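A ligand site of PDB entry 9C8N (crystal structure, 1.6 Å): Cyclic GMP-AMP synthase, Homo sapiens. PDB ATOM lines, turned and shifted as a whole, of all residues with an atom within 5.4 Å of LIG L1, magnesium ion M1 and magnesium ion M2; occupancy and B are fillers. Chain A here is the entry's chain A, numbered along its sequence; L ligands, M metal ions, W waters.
NZ of Lys 259 lies within salt-bridge range of O1 of LIG L1, at 2.8 Å.
The side-chain hydroxyl of Ser 280 is in hydrogen-bond range of an oxygen (O2) of LIG L1 (3.0 Å).
The side-chain carboxylate of Glu 228 is in hydrogen-bond range of an oxygen (O12) of LIG L1, 2.8 Å away.
OG of Ser 225 is in hydrogen-bond range of O12 of LIG L1 (2.8 Å).
The side-chain hydroxyl (OG) of Ser 58 lies within hydrogen-bond range of an oxygen (O1) of LIG L1 (2.6 Å).
The side-chain amino group (NZ) of Lys 284 lies within hydrogen-bond range of an oxygen (O11) of LIG L1, 3.0 Å away.
An oxygen (O5) of LIG L1 sits close to the backbone NH (N) of Ser 58 (3.0 Å).
N of Asp 164 is in hydrogen-bond range of O of Phe 71.
N of Tyr 281 lies close to OG of Ser 279.
The backbone carbonyl oxygen (O) of Ser 58 sits at hydrogen-bond distance from the backbone NH (N) of Lys 64.
The side-chain amino group of Lys 284 is in salt-bridge range of the side-chain carboxylate of Glu 61, at 2.7 Å.
The backbone NH (N) of Val 63 lies within hydrogen-bond range of the backbone carbonyl oxygen (O) of Ser 58 (2.9 Å).
The backbone carbonyl oxygen of Asp 72 sits at hydrogen-bond distance from the backbone NH of Thr 56, at 2.9 Å.
The side-chain hydroxyl (OG) of Ser 225 sits at hydrogen-bond distance from the side-chain hydroxyl (OG) of Ser 223, 3.2 Å away.
OH of Tyr 281 lies within hydrogen-bond range of OE2 of Glu 228.
Merely in contact with LIG L1: Tyr 281 (3.3 Å), Gly 57 (3.6 Å), Arg 221 (3.7 Å) and Lys 64 (3.96 Å).
Within 4 Å of LIG L1: Gly 57, Ser 58, Lys 64, Glu 70, Asp 72, Arg 221, Ser 225, Glu 228, Lys 259, Ser 280, Tyr 281 and Lys 284.
Three residues have an atom within 4 Å of magnesium ion M1: Glu 70, Asp 72 and Asp 164.
The nearest printed residue that does not touch magnesium ion M1 is Phe 71 (4.8 Å).
Merely in contact with magnesium ion M2: Ser 58.
Of the 23 residues printed, 3 come within 4 Å of magnesium ion M2.
Magnesium ion M1 is bound by OD1 of Asp 72 (2.0 Å).
The side-chain carboxylate (OE2) of Glu 70 binds magnesium ion M1.
OD2 of Asp 164 is bound to magnesium ion M1.
Magnesium ion M1 is bound by O2 of LG2 L2, 2.1 Å away.
O1 of LG2 L2 is bound to magnesium ion M1 (2.1 Å).
O7 of LIG L1 is bound to magnesium ion M1 (2.2 Å).
Magnesium ion M2 is bound by OE1 of Glu 70 (2.1 Å), OD2 of Asp 72 (2.1 Å), O5 of LIG L1 (2.1 Å), water W6 (2.1 Å), O3 of LIG L1 (2.1 Å) and O7 of LIG L1 (2.3 Å).
Water W8 lies within hydrogen-bond range of O2 of LIG L1 (2.6 Å) and OG of Ser 280 (3.2 Å).
Water W10 lies within hydrogen-bond range of a nitrogen (N6) of LIG L1, the side-chain hydroxyl (OG) of Ser 225 and the side-chain hydroxyl (OG) of Ser 223.
Water W3 lies within hydrogen-bond range of a nitrogen (N3) of LIG L1 (2.8 Å) and the side-chain hydroxyl of Ser 279 (2.9 Å).
Water W4 lies within hydrogen-bond range of an oxygen (O4) of LIG L1 (2.8 Å), the backbone NH of Tyr 281 (3.1 Å) and the side-chain hydroxyl of Ser 280 (3.2 Å).
Water W2 lies within hydrogen-bond range of an oxygen (O6) of LIG L1 (2.8 Å), the side-chain hydroxyl (OG) of Ser 280 (2.9 Å) and the backbone NH (N) of Tyr 281 (3.0 Å).
Water W7 lies within hydrogen-bond range of an oxygen (O1) of LIG L1 (2.9 Å), the side-chain amino group of Lys 64 (2.9 Å) and the backbone NH of Ile 65 (3.0 Å).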
ATOM      1  N   THR A  56      28.101   1.466  27.785  1.00  0.00           N
ATOM      2  CA  THR A  56      27.148   0.896  26.814  1.00  0.00           C
ATOM      3  C   THR A  56      25.874   1.696  26.841  1.00  0.00           C
ATOM      4  O   THR A  56      25.699   2.598  27.670  1.00  0.00           O
ATOM      5  CB  THR A  56      26.792  -0.583  27.174  1.00  0.00           C
ATOM      6  OG1 THR A  56      26.119  -0.611  28.443  1.00  0.00           O
ATOM      7  CG2 THR A  56      28.052  -1.433  27.194  1.00  0.00           C
ATOM      8  N   GLY A  57      24.939   1.336  25.951  1.00  0.00           N
ATOM      9  CA  GLY A  57      23.621   1.952  26.075  1.00  0.00           C
ATOM     10  C   GLY A  57      23.542   3.365  25.502  1.00  0.00           C
ATOM     11  O   GLY A  57      24.470   3.910  24.896  1.00  0.00           O
ATOM     12  N   SER A  58      22.355   3.961  25.687  1.00  0.00           N
ATOM     13  CA  SER A  58      22.010   5.111  24.846  1.00  0.00           C
ATOM     14  C   SER A  58      22.875   6.337  25.119  1.00  0.00           C
ATOM     15  O   SER A  58      23.088   7.109  24.191  1.00  0.00           O
ATOM     16  CB  SER A  58      20.548   5.471  25.012  1.00  0.00           C
ATOM     17  OG  SER A  58      20.253   5.948  26.333  1.00  0.00           O
ATOM     18  N   TYR A  59      23.341   6.547  26.373  1.00  0.00           N
ATOM     19  CA  TYR A  59      24.166   7.729  26.608  1.00  0.00           C
ATOM     20  C   TYR A  59      25.441   7.650  25.767  1.00  0.00           C
ATOM     21  O   TYR A  59      25.793   8.604  25.063  1.00  0.00           O
ATOM     22  CB  TYR A  59      24.541   7.832  28.102  1.00  0.00           C
ATOM     23  CG  TYR A  59      25.371   9.076  28.383  1.00  0.00           C
ATOM     24  CD1 TYR A  59      24.794  10.286  28.658  1.00  0.00           C
ATOM     25  CD2 TYR A  59      26.754   8.985  28.385  1.00  0.00           C
ATOM     26  CE1 TYR A  59      25.534  11.395  28.895  1.00  0.00           C
ATOM     27  CE2 TYR A  59      27.559  10.130  28.586  1.00  0.00           C
ATOM     28  CZ  TYR A  59      26.882  11.317  28.848  1.00  0.00           C
ATOM     29  OH  TYR A  59      27.624  12.465  29.106  1.00  0.00           O
ATOM     30  N   GLU A  61      25.948   5.931  23.126  1.00  0.00           N
ATOM     31  CA  GLU A  61      25.555   5.910  21.705  1.00  0.00           C
ATOM     32  C   GLU A  61      25.008   7.239  21.239  1.00  0.00           C
ATOM     33  O   GLU A  61      24.624   7.384  20.083  1.00  0.00           O
ATOM     34  CB  GLU A  61      24.473   4.831  21.503  1.00  0.00           C
ATOM     35  CG  GLU A  61      25.013   3.388  21.760  1.00  0.00           C
ATOM     36  CD  GLU A  61      23.893   2.395  22.009  1.00  0.00           C
ATOM     37  OE1 GLU A  61      22.751   2.796  22.304  1.00  0.00           O
ATOM     38  OE2 GLU A  61      24.183   1.179  21.883  1.00  0.00           O
ATOM     39  N   VAL A  63      22.239   8.580  21.828  1.00  0.00           N
ATOM     40  CA  VAL A  63      20.802   8.593  21.535  1.00  0.00           C
ATOM     41  C   VAL A  63      19.972   8.660  22.805  1.00  0.00           C
ATOM     42  O   VAL A  63      18.744   8.508  22.758  1.00  0.00           O
ATOM     43  CB  VAL A  63      20.385   7.406  20.646  1.00  0.00           C
ATOM     44  CG1 VAL A  63      21.031   7.578  19.237  1.00  0.00           C
ATOM     45  CG2 VAL A  63      20.773   6.077  21.233  1.00  0.00           C
ATOM     46  N   LYS A  64      20.603   9.001  23.943  1.00  0.00           N
ATOM     47  CA  LYS A  64      19.802   9.279  25.142  1.00  0.00           C
ATOM     48  C   LYS A  64      18.969  10.535  24.881  1.00  0.00           C
ATOM     49  O   LYS A  64      19.501  11.508  24.349  1.00  0.00           O
ATOM     50  CB  LYS A  64      20.765   9.495  26.330  1.00  0.00           C
ATOM     51  CG  LYS A  64      20.050   9.782  27.691  1.00  0.00           C
ATOM     52  CD  LYS A  64      19.551   8.524  28.330  1.00  0.00           C
ATOM     53  CE  LYS A  64      18.721   8.776  29.587  1.00  0.00           C
ATOM     54  NZ  LYS A  64      17.395   9.439  29.261  1.00  0.00           N
ATOM     55  N   ILE A  65      17.684  10.521  25.313  1.00  0.00           N
ATOM     56  CA  ILE A  65      16.799  11.671  25.092  1.00  0.00           C
ATOM     57  C   ILE A  65      16.441  12.306  26.427  1.00  0.00           C
ATOM     58  O   ILE A  65      16.448  11.678  27.491  1.00  0.00           O
ATOM     59  CB  ILE A  65      15.535  11.280  24.261  1.00  0.00           C
ATOM     60  CG1 ILE A  65      14.739  10.199  24.988  1.00  0.00           C
ATOM     61  CG2 ILE A  65      15.970  10.915  22.817  1.00  0.00           C
ATOM     62  CD1 ILE A  65      13.413   9.884  24.229  1.00  0.00           C
ATOM     63  N   GLU A  70      20.209   8.376  32.929  1.00  0.00           N
ATOM     64  CA  GLU A  70      20.300   6.911  32.996  1.00  0.00           C
ATOM     65  C   GLU A  70      21.465   6.447  32.152  1.00  0.00           C
ATOM     66  O   GLU A  70      21.531   6.695  30.926  1.00  0.00           O
ATOM     67  CB  GLU A  70      19.001   6.252  32.501  1.00  0.00           C
ATOM     68  CG  GLU A  70      18.808   4.815  33.029  1.00  0.00           C
ATOM     69  CD  GLU A  70      19.279   3.725  32.078  1.00  0.00           C
ATOM     70  OE1 GLU A  70      19.723   4.048  30.961  1.00  0.00           O
ATOM     71  OE2 GLU A  70      19.169   2.505  32.463  1.00  0.00           O
ATOM     72  N   PHE A  71      22.388   5.761  32.818  1.00  0.00           N
ATOM     73  CA  PHE A  71      23.657   5.329  32.231  1.00  0.00           C
ATOM     74  C   PHE A  71      23.775   3.824  32.389  1.00  0.00           C
ATOM     75  O   PHE A  71      23.377   3.287  33.418  1.00  0.00           O
ATOM     76  CB  PHE A  71      24.864   5.987  32.961  1.00  0.00           C
ATOM     77  CG  PHE A  71      24.997   7.448  32.768  1.00  0.00           C
ATOM     78  CD1 PHE A  71      24.098   8.349  33.377  1.00  0.00           C
ATOM     79  CD2 PHE A  71      26.080   7.928  32.033  1.00  0.00           C
ATOM     80  CE1 PHE A  71      24.241   9.728  33.183  1.00  0.00           C
ATOM     81  CE2 PHE A  71      26.223   9.315  31.816  1.00  0.00           C
ATOM     82  CZ  PHE A  71      25.299  10.196  32.417  1.00  0.00           C
ATOM     83  N   ASP A  72      24.406   3.165  31.419  1.00  0.00           N
ATOM     84  CA  ASP A  72      24.583   1.715  31.423  1.00  0.00           C
ATOM     85  C   ASP A  72      26.043   1.365  31.277  1.00  0.00           C
ATOM     86  O   ASP A  72      26.703   1.854  30.349  1.00  0.00           O
ATOM     87  CB  ASP A  72      23.781   1.118  30.265  1.00  0.00           C
ATOM     88  CG  ASP A  72      22.312   1.489  30.336  1.00  0.00           C
ATOM     89  OD1 ASP A  72      21.611   0.957  31.225  1.00  0.00           O
ATOM     90  OD2 ASP A  72      21.913   2.379  29.529  1.00  0.00           O
ATOM     91  N   ASP A 164      22.930   1.470  35.654  1.00  0.00           N
ATOM     92  CA  ASP A 164      22.872   0.004  35.579  1.00  0.00           C
ATOM     93  C   ASP A 164      24.284  -0.525  35.428  1.00  0.00           C
ATOM     94  O   ASP A 164      24.985  -0.151  34.475  1.00  0.00           O
ATOM     95  CB  ASP A 164      22.063  -0.479  34.372  1.00  0.00           C
ATOM     96  CG  ASP A 164      20.593  -0.240  34.555  1.00  0.00           C
ATOM     97  OD1 ASP A 164      20.058  -0.454  35.677  1.00  0.00           O
ATOM     98  OD2 ASP A 164      19.926   0.146  33.582  1.00  0.00           O
ATOM     99  N   ARG A 221      23.394 -15.087  29.709  1.00  0.00           N
ATOM    100  CA  ARG A 221      22.775 -14.592  28.487  1.00  0.00           C
ATOM    101  C   ARG A 221      23.815 -13.889  27.628  1.00  0.00           C
ATOM    102  O   ARG A 221      24.643 -13.130  28.152  1.00  0.00           O
ATOM    103  CB  ARG A 221      21.657 -13.662  28.913  1.00  0.00           C
ATOM    104  CG  ARG A 221      21.112 -12.783  27.849  1.00  0.00           C
ATOM    105  CD  ARG A 221      20.278 -13.551  26.922  1.00  0.00           C
ATOM    106  NE  ARG A 221      19.851 -12.712  25.809  1.00  0.00           N
ATOM    107  CZ  ARG A 221      18.647 -12.182  25.632  1.00  0.00           C
ATOM    108  NH1 ARG A 221      17.655 -12.357  26.509  1.00  0.00           N
ATOM    109  NH2 ARG A 221      18.410 -11.473  24.542  1.00  0.00           N
ATOM    110  N   SER A 223      25.450 -11.229  25.280  1.00  0.00           N
ATOM    111  CA  SER A 223      25.269  -9.799  25.106  1.00  0.00           C
ATOM    112  C   SER A 223      26.277  -9.260  24.094  1.00  0.00           C
ATOM    113  O   SER A 223      27.486  -9.557  24.162  1.00  0.00           O
ATOM    114  CB  SER A 223      25.427  -9.058  26.434  1.00  0.00           C
ATOM    115  OG  SER A 223      25.356  -7.645  26.244  1.00  0.00           O
ATOM    116  N   SER A 225      26.172  -5.716  23.489  1.00  0.00           N
ATOM    117  CA  SER A 225      25.964  -4.281  23.673  1.00  0.00           C
ATOM    118  C   SER A 225      27.122  -3.475  23.129  1.00  0.00           C
ATOM    119  O   SER A 225      26.936  -2.357  22.631  1.00  0.00           O
ATOM    120  CB  SER A 225      25.789  -3.928  25.162  1.00  0.00           C
ATOM    121  OG  SER A 225      24.663  -4.558  25.691  1.00  0.00           O
ATOM    122  N   GLU A 228      26.565  -3.125  19.422  1.00  0.00           N
ATOM    123  CA  GLU A 228      25.508  -2.125  19.190  1.00  0.00           C
ATOM    124  C   GLU A 228      26.073  -0.706  19.230  1.00  0.00           C
ATOM    125  O   GLU A 228      25.681   0.153  18.413  1.00  0.00           O
ATOM    126  CB  GLU A 228      24.392  -2.280  20.231  1.00  0.00           C
ATOM    127  CG  GLU A 228      23.757  -3.656  20.089  1.00  0.00           C
ATOM    128  CD  GLU A 228      22.781  -3.983  21.189  1.00  0.00           C
ATOM    129  OE1 GLU A 228      22.436  -3.120  22.031  1.00  0.00           O
ATOM    130  OE2 GLU A 228      22.335  -5.135  21.238  1.00  0.00           O
ATOM    131  N   LYS A 259      12.142   5.972  20.153  1.00  0.00           N
ATOM    132  CA  LYS A 259      12.299   5.826  21.610  1.00  0.00           C
ATOM    133  C   LYS A 259      11.296   6.705  22.343  1.00  0.00           C
ATOM    134  O   LYS A 259      10.642   6.251  23.299  1.00  0.00           O
ATOM    135  CB  LYS A 259      13.737   6.201  22.033  1.00  0.00           C
ATOM    136  CG  LYS A 259      14.798   5.186  21.637  1.00  0.00           C
ATOM    137  CD  LYS A 259      16.199   5.807  21.773  1.00  0.00           C
ATOM    138  CE  LYS A 259      16.488   6.264  23.196  1.00  0.00           C
ATOM    139  NZ  LYS A 259      16.309   5.154  24.133  1.00  0.00           N
ATOM    140  N   SER A 279      10.031  -2.400  25.698  1.00  0.00           N
ATOM    141  CA  SER A 279      11.140  -1.594  26.166  1.00  0.00           C
ATOM    142  C   SER A 279      11.789  -0.899  24.992  1.00  0.00           C
ATOM    143  O   SER A 279      11.577  -1.221  23.809  1.00  0.00           O
ATOM    144  CB  SER A 279      12.198  -2.436  26.918  1.00  0.00           C
ATOM    145  OG  SER A 279      13.010  -3.123  25.982  1.00  0.00           O
ATOM    146  N   SER A 280      12.674   0.063  25.326  1.00  0.00           N
ATOM    147  CA  SER A 280      13.390   0.739  24.256  1.00  0.00           C
ATOM    148  C   SER A 280      14.257  -0.206  23.442  1.00  0.00           C
ATOM    149  O   SER A 280      14.540   0.116  22.286  1.00  0.00           O
ATOM    150  CB  SER A 280      14.228   1.892  24.814  1.00  0.00           C
ATOM    151  OG  SER A 280      15.223   1.432  25.668  1.00  0.00           O
ATOM    152  N   TYR A 281      14.606  -1.391  23.992  1.00  0.00           N
ATOM    153  CA  TYR A 281      15.387  -2.339  23.181  1.00  0.00           C
ATOM    154  C   TYR A 281      14.561  -2.901  22.034  1.00  0.00           C
ATOM    155  O   TYR A 281      15.119  -3.292  21.001  1.00  0.00           O
ATOM    156  CB  TYR A 281      15.914  -3.481  24.064  1.00  0.00           C
ATOM    157  CG  TYR A 281      16.996  -4.290  23.345  1.00  0.00           C
ATOM    158  CD1 TYR A 281      18.261  -3.722  23.087  1.00  0.00           C
ATOM    159  CD2 TYR A 281      16.752  -5.583  22.934  1.00  0.00           C
ATOM    160  CE1 TYR A 281      19.225  -4.401  22.429  1.00  0.00           C
ATOM    161  CE2 TYR A 281      17.806  -6.283  22.270  1.00  0.00           C
ATOM    162  CZ  TYR A 281      19.008  -5.672  22.039  1.00  0.00           C
ATOM    163  OH  TYR A 281      19.948  -6.404  21.380  1.00  0.00           O
ATOM    164  N   LYS A 284      15.079  -0.274  19.524  1.00  0.00           N
ATOM    165  CA  LYS A 284      16.450  -0.307  19.047  1.00  0.00           C
ATOM    166  C   LYS A 284      16.661  -1.439  18.046  1.00  0.00           C
ATOM    167  O   LYS A 284      17.277  -1.247  16.977  1.00  0.00           O
ATOM    168  CB  LYS A 284      17.383  -0.478  20.245  1.00  0.00           C
ATOM    169  CG  LYS A 284      18.827  -0.182  19.908  1.00  0.00           C
ATOM    170  CD  LYS A 284      19.685  -0.489  21.119  1.00  0.00           C
ATOM    171  CE  LYS A 284      21.138  -0.012  20.841  1.00  0.00           C
ATOM    172  NZ  LYS A 284      22.009  -0.420  22.011  1.00  0.00           N
ATOM    173  N   ASN A 327      16.199 -10.924  17.449  1.00  0.00           N
ATOM    174  CA  ASN A 327      17.394 -10.306  17.963  1.00  0.00           C
ATOM    175  C   ASN A 327      18.368 -10.066  16.801  1.00  0.00           C
ATOM    176  O   ASN A 327      18.535 -10.930  15.958  1.00  0.00           O
ATOM    177  CB  ASN A 327      17.983 -11.202  19.054  1.00  0.00           C
ATOM    178  CG  ASN A 327      19.194 -10.576  19.710  1.00  0.00           C
ATOM    179  OD1 ASN A 327      20.230 -10.528  19.090  1.00  0.00           O
ATOM    180  ND2 ASN A 327      19.057 -10.085  20.945  1.00  0.00           N
ATOM    181  N   LEU A 335      12.222 -11.665  19.897  1.00  0.00           N
ATOM    182  CA  LEU A 335      11.782 -10.821  21.007  1.00  0.00           C
ATOM    183  C   LEU A 335      10.279 -10.697  21.077  1.00  0.00           C
ATOM    184  O   LEU A 335       9.747 -10.398  22.146  1.00  0.00           O
ATOM    185  CB  LEU A 335      12.389  -9.394  20.888  1.00  0.00           C
ATOM    186  CG  LEU A 335      13.890  -9.173  20.710  1.00  0.00           C
ATOM    187  CD1 LEU A 335      14.243  -7.757  21.159  1.00  0.00           C
ATOM    188  CD2 LEU A 335      14.728 -10.225  21.382  1.00  0.00           C
HETATM  189  P1  LIG L   1      17.408   4.168  27.238  1.00  0.00           P
HETATM  190  O1  LIG L   1      17.691   5.491  26.582  1.00  0.00           O
HETATM  191  O2  LIG L   1      15.958   3.777  27.376  1.00  0.00           O
HETATM  192  O3  LIG L   1      18.190   3.969  28.510  1.00  0.00           O
HETATM  193  P2  LIG L   1      19.220   2.084  26.209  1.00  0.00           P
HETATM  194  O4  LIG L   1      19.717   1.329  25.033  1.00  0.00           O
HETATM  195  O5  LIG L   1      20.265   2.390  27.233  1.00  0.00           O
HETATM  196  N1  LIG L   1      18.001   3.124  26.003  1.00  0.00           N
HETATM  197  P3  LIG L   1      18.494   0.325  28.560  1.00  0.00           P
HETATM  198  O6  LIG L   1      17.323  -0.435  29.032  1.00  0.00           O
HETATM  199  O7  LIG L   1      19.249   1.138  29.552  1.00  0.00           O
HETATM  200  O8  LIG L   1      18.409   0.765  27.091  1.00  0.00           O
HETATM  201  O9  LIG L   1      19.662  -1.037  28.332  1.00  0.00           O
HETATM  202  C1  LIG L   1      20.944  -0.724  28.155  1.00  0.00           C
HETATM  203  C2  LIG L   1      21.579  -1.678  27.145  1.00  0.00           C
HETATM  204  O10 LIG L   1      21.390  -3.003  27.616  1.00  0.00           O
HETATM  205  C3  LIG L   1      20.867  -1.623  25.783  1.00  0.00           C
HETATM  206  O11 LIG L   1      21.408  -0.670  24.979  1.00  0.00           O
HETATM  207  C4  LIG L   1      21.247  -3.035  25.243  1.00  0.00           C
HETATM  208  O12 LIG L   1      22.556  -2.967  24.812  1.00  0.00           O
HETATM  209  C5  LIG L   1      21.198  -3.868  26.547  1.00  0.00           C
HETATM  210  N2  LIG L   1      19.878  -4.449  26.648  1.00  0.00           N
HETATM  211  C6  LIG L   1      18.719  -3.948  27.267  1.00  0.00           C
HETATM  212  N3  LIG L   1      17.698  -4.775  27.090  1.00  0.00           N
HETATM  213  C7  LIG L   1      18.177  -5.821  26.346  1.00  0.00           C
HETATM  214  C8  LIG L   1      17.604  -6.971  25.852  1.00  0.00           C
HETATM  215  N4  LIG L   1      16.281  -7.237  26.097  1.00  0.00           N
HETATM  216  N5  LIG L   1      18.309  -7.852  25.132  1.00  0.00           N
HETATM  217  C9  LIG L   1      19.593  -7.531  24.932  1.00  0.00           C
HETATM  218  N6  LIG L   1      20.291  -6.482  25.336  1.00  0.00           N
HETATM  219  C10 LIG L   1      19.544  -5.634  26.039  1.00  0.00           C
HETATM  220  C1  LG2 L   2      21.210  -8.247  28.071  1.00  0.00           C
HETATM  221  C2  LG2 L   2      21.600  -6.178  29.262  1.00  0.00           C
HETATM  222  C3  LG2 L   2      19.469  -5.263  30.444  1.00  0.00           C
HETATM  223  C4  LG2 L   2      16.505   0.991  32.248  1.00  0.00           C
HETATM  224  C5  LG2 L   2      17.345  -1.185  32.064  1.00  0.00           C
HETATM  225  C6  LG2 L   2      18.590  -1.915  31.521  1.00  0.00           C
HETATM  226  C7  LG2 L   2      17.492  -4.047  32.059  1.00  0.00           C
HETATM  227  C8  LG2 L   2      17.008  -5.131  31.101  1.00  0.00           C
HETATM  228  C9  LG2 L   2      18.183  -5.759  30.424  1.00  0.00           C
HETATM  229  C10 LG2 L   2      19.426  -7.239  29.246  1.00  0.00           C
HETATM  230  C11 LG2 L   2      19.920  -8.232  28.470  1.00  0.00           C
HETATM  231  C12 LG2 L   2      22.112  -7.169  28.461  1.00  0.00           C
HETATM  232  C13 LG2 L   2      20.281  -6.142  29.653  1.00  0.00           C
HETATM  233  C14 LG2 L   2      19.823  -3.946  31.063  1.00  0.00           C
HETATM  234  C15 LG2 L   2      20.899  -4.137  32.220  1.00  0.00           C
HETATM  235  N1  LG2 L   2      18.635  -3.245  31.496  1.00  0.00           N
HETATM  236  N2  LG2 L   2      18.147  -6.986  29.723  1.00  0.00           N
HETATM  237  O1  LG2 L   2      17.622   0.179  31.959  1.00  0.00           O
HETATM  238  O2  LG2 L   2      19.589  -1.256  31.175  1.00  0.00           O
HETATM  239 CL1  LG2 L   2      21.868  -9.471  27.022  1.00  0.00          CL
HETATM  240 CL2  LG2 L   2      18.809  -9.484  27.999  1.00  0.00          CL
HETATM  241 MG    MG M   1      19.663   0.750  31.633  1.00  0.00          MG
HETATM  242 MG    MG M   2      20.061   3.197  29.126  1.00  0.00          MG
HETATM  243  O   HOH W   1      16.581   4.962  30.537  1.00  0.00           O
HETATM  244  O   HOH W   2      15.902  -1.148  26.686  1.00  0.00           O
HETATM  245  O   HOH W   3      15.113  -3.959  27.785  1.00  0.00           O
HETATM  246  O   HOH W   4      17.525  -0.239  24.173  1.00  0.00           O
HETATM  247  O   HOH W   5      14.325  -9.765  24.788  1.00  0.00           O
HETATM  248  O   HOH W   6      21.096   4.984  28.739  1.00  0.00           O
HETATM  249  O   HOH W   7      16.553   8.109  26.768  1.00  0.00           O
HETATM  250  O   HOH W   8      15.241   1.762  28.862  1.00  0.00           O
HETATM  251  O   HOH W   9      24.231  -2.703  29.123  1.00  0.00           O
HETATM  252  O   HOH W  10      23.023  -6.710  24.869  1.00  0.00           O
HETATM  253  O   HOH W  11      17.138  -9.599  23.181  1.00  0.00           O
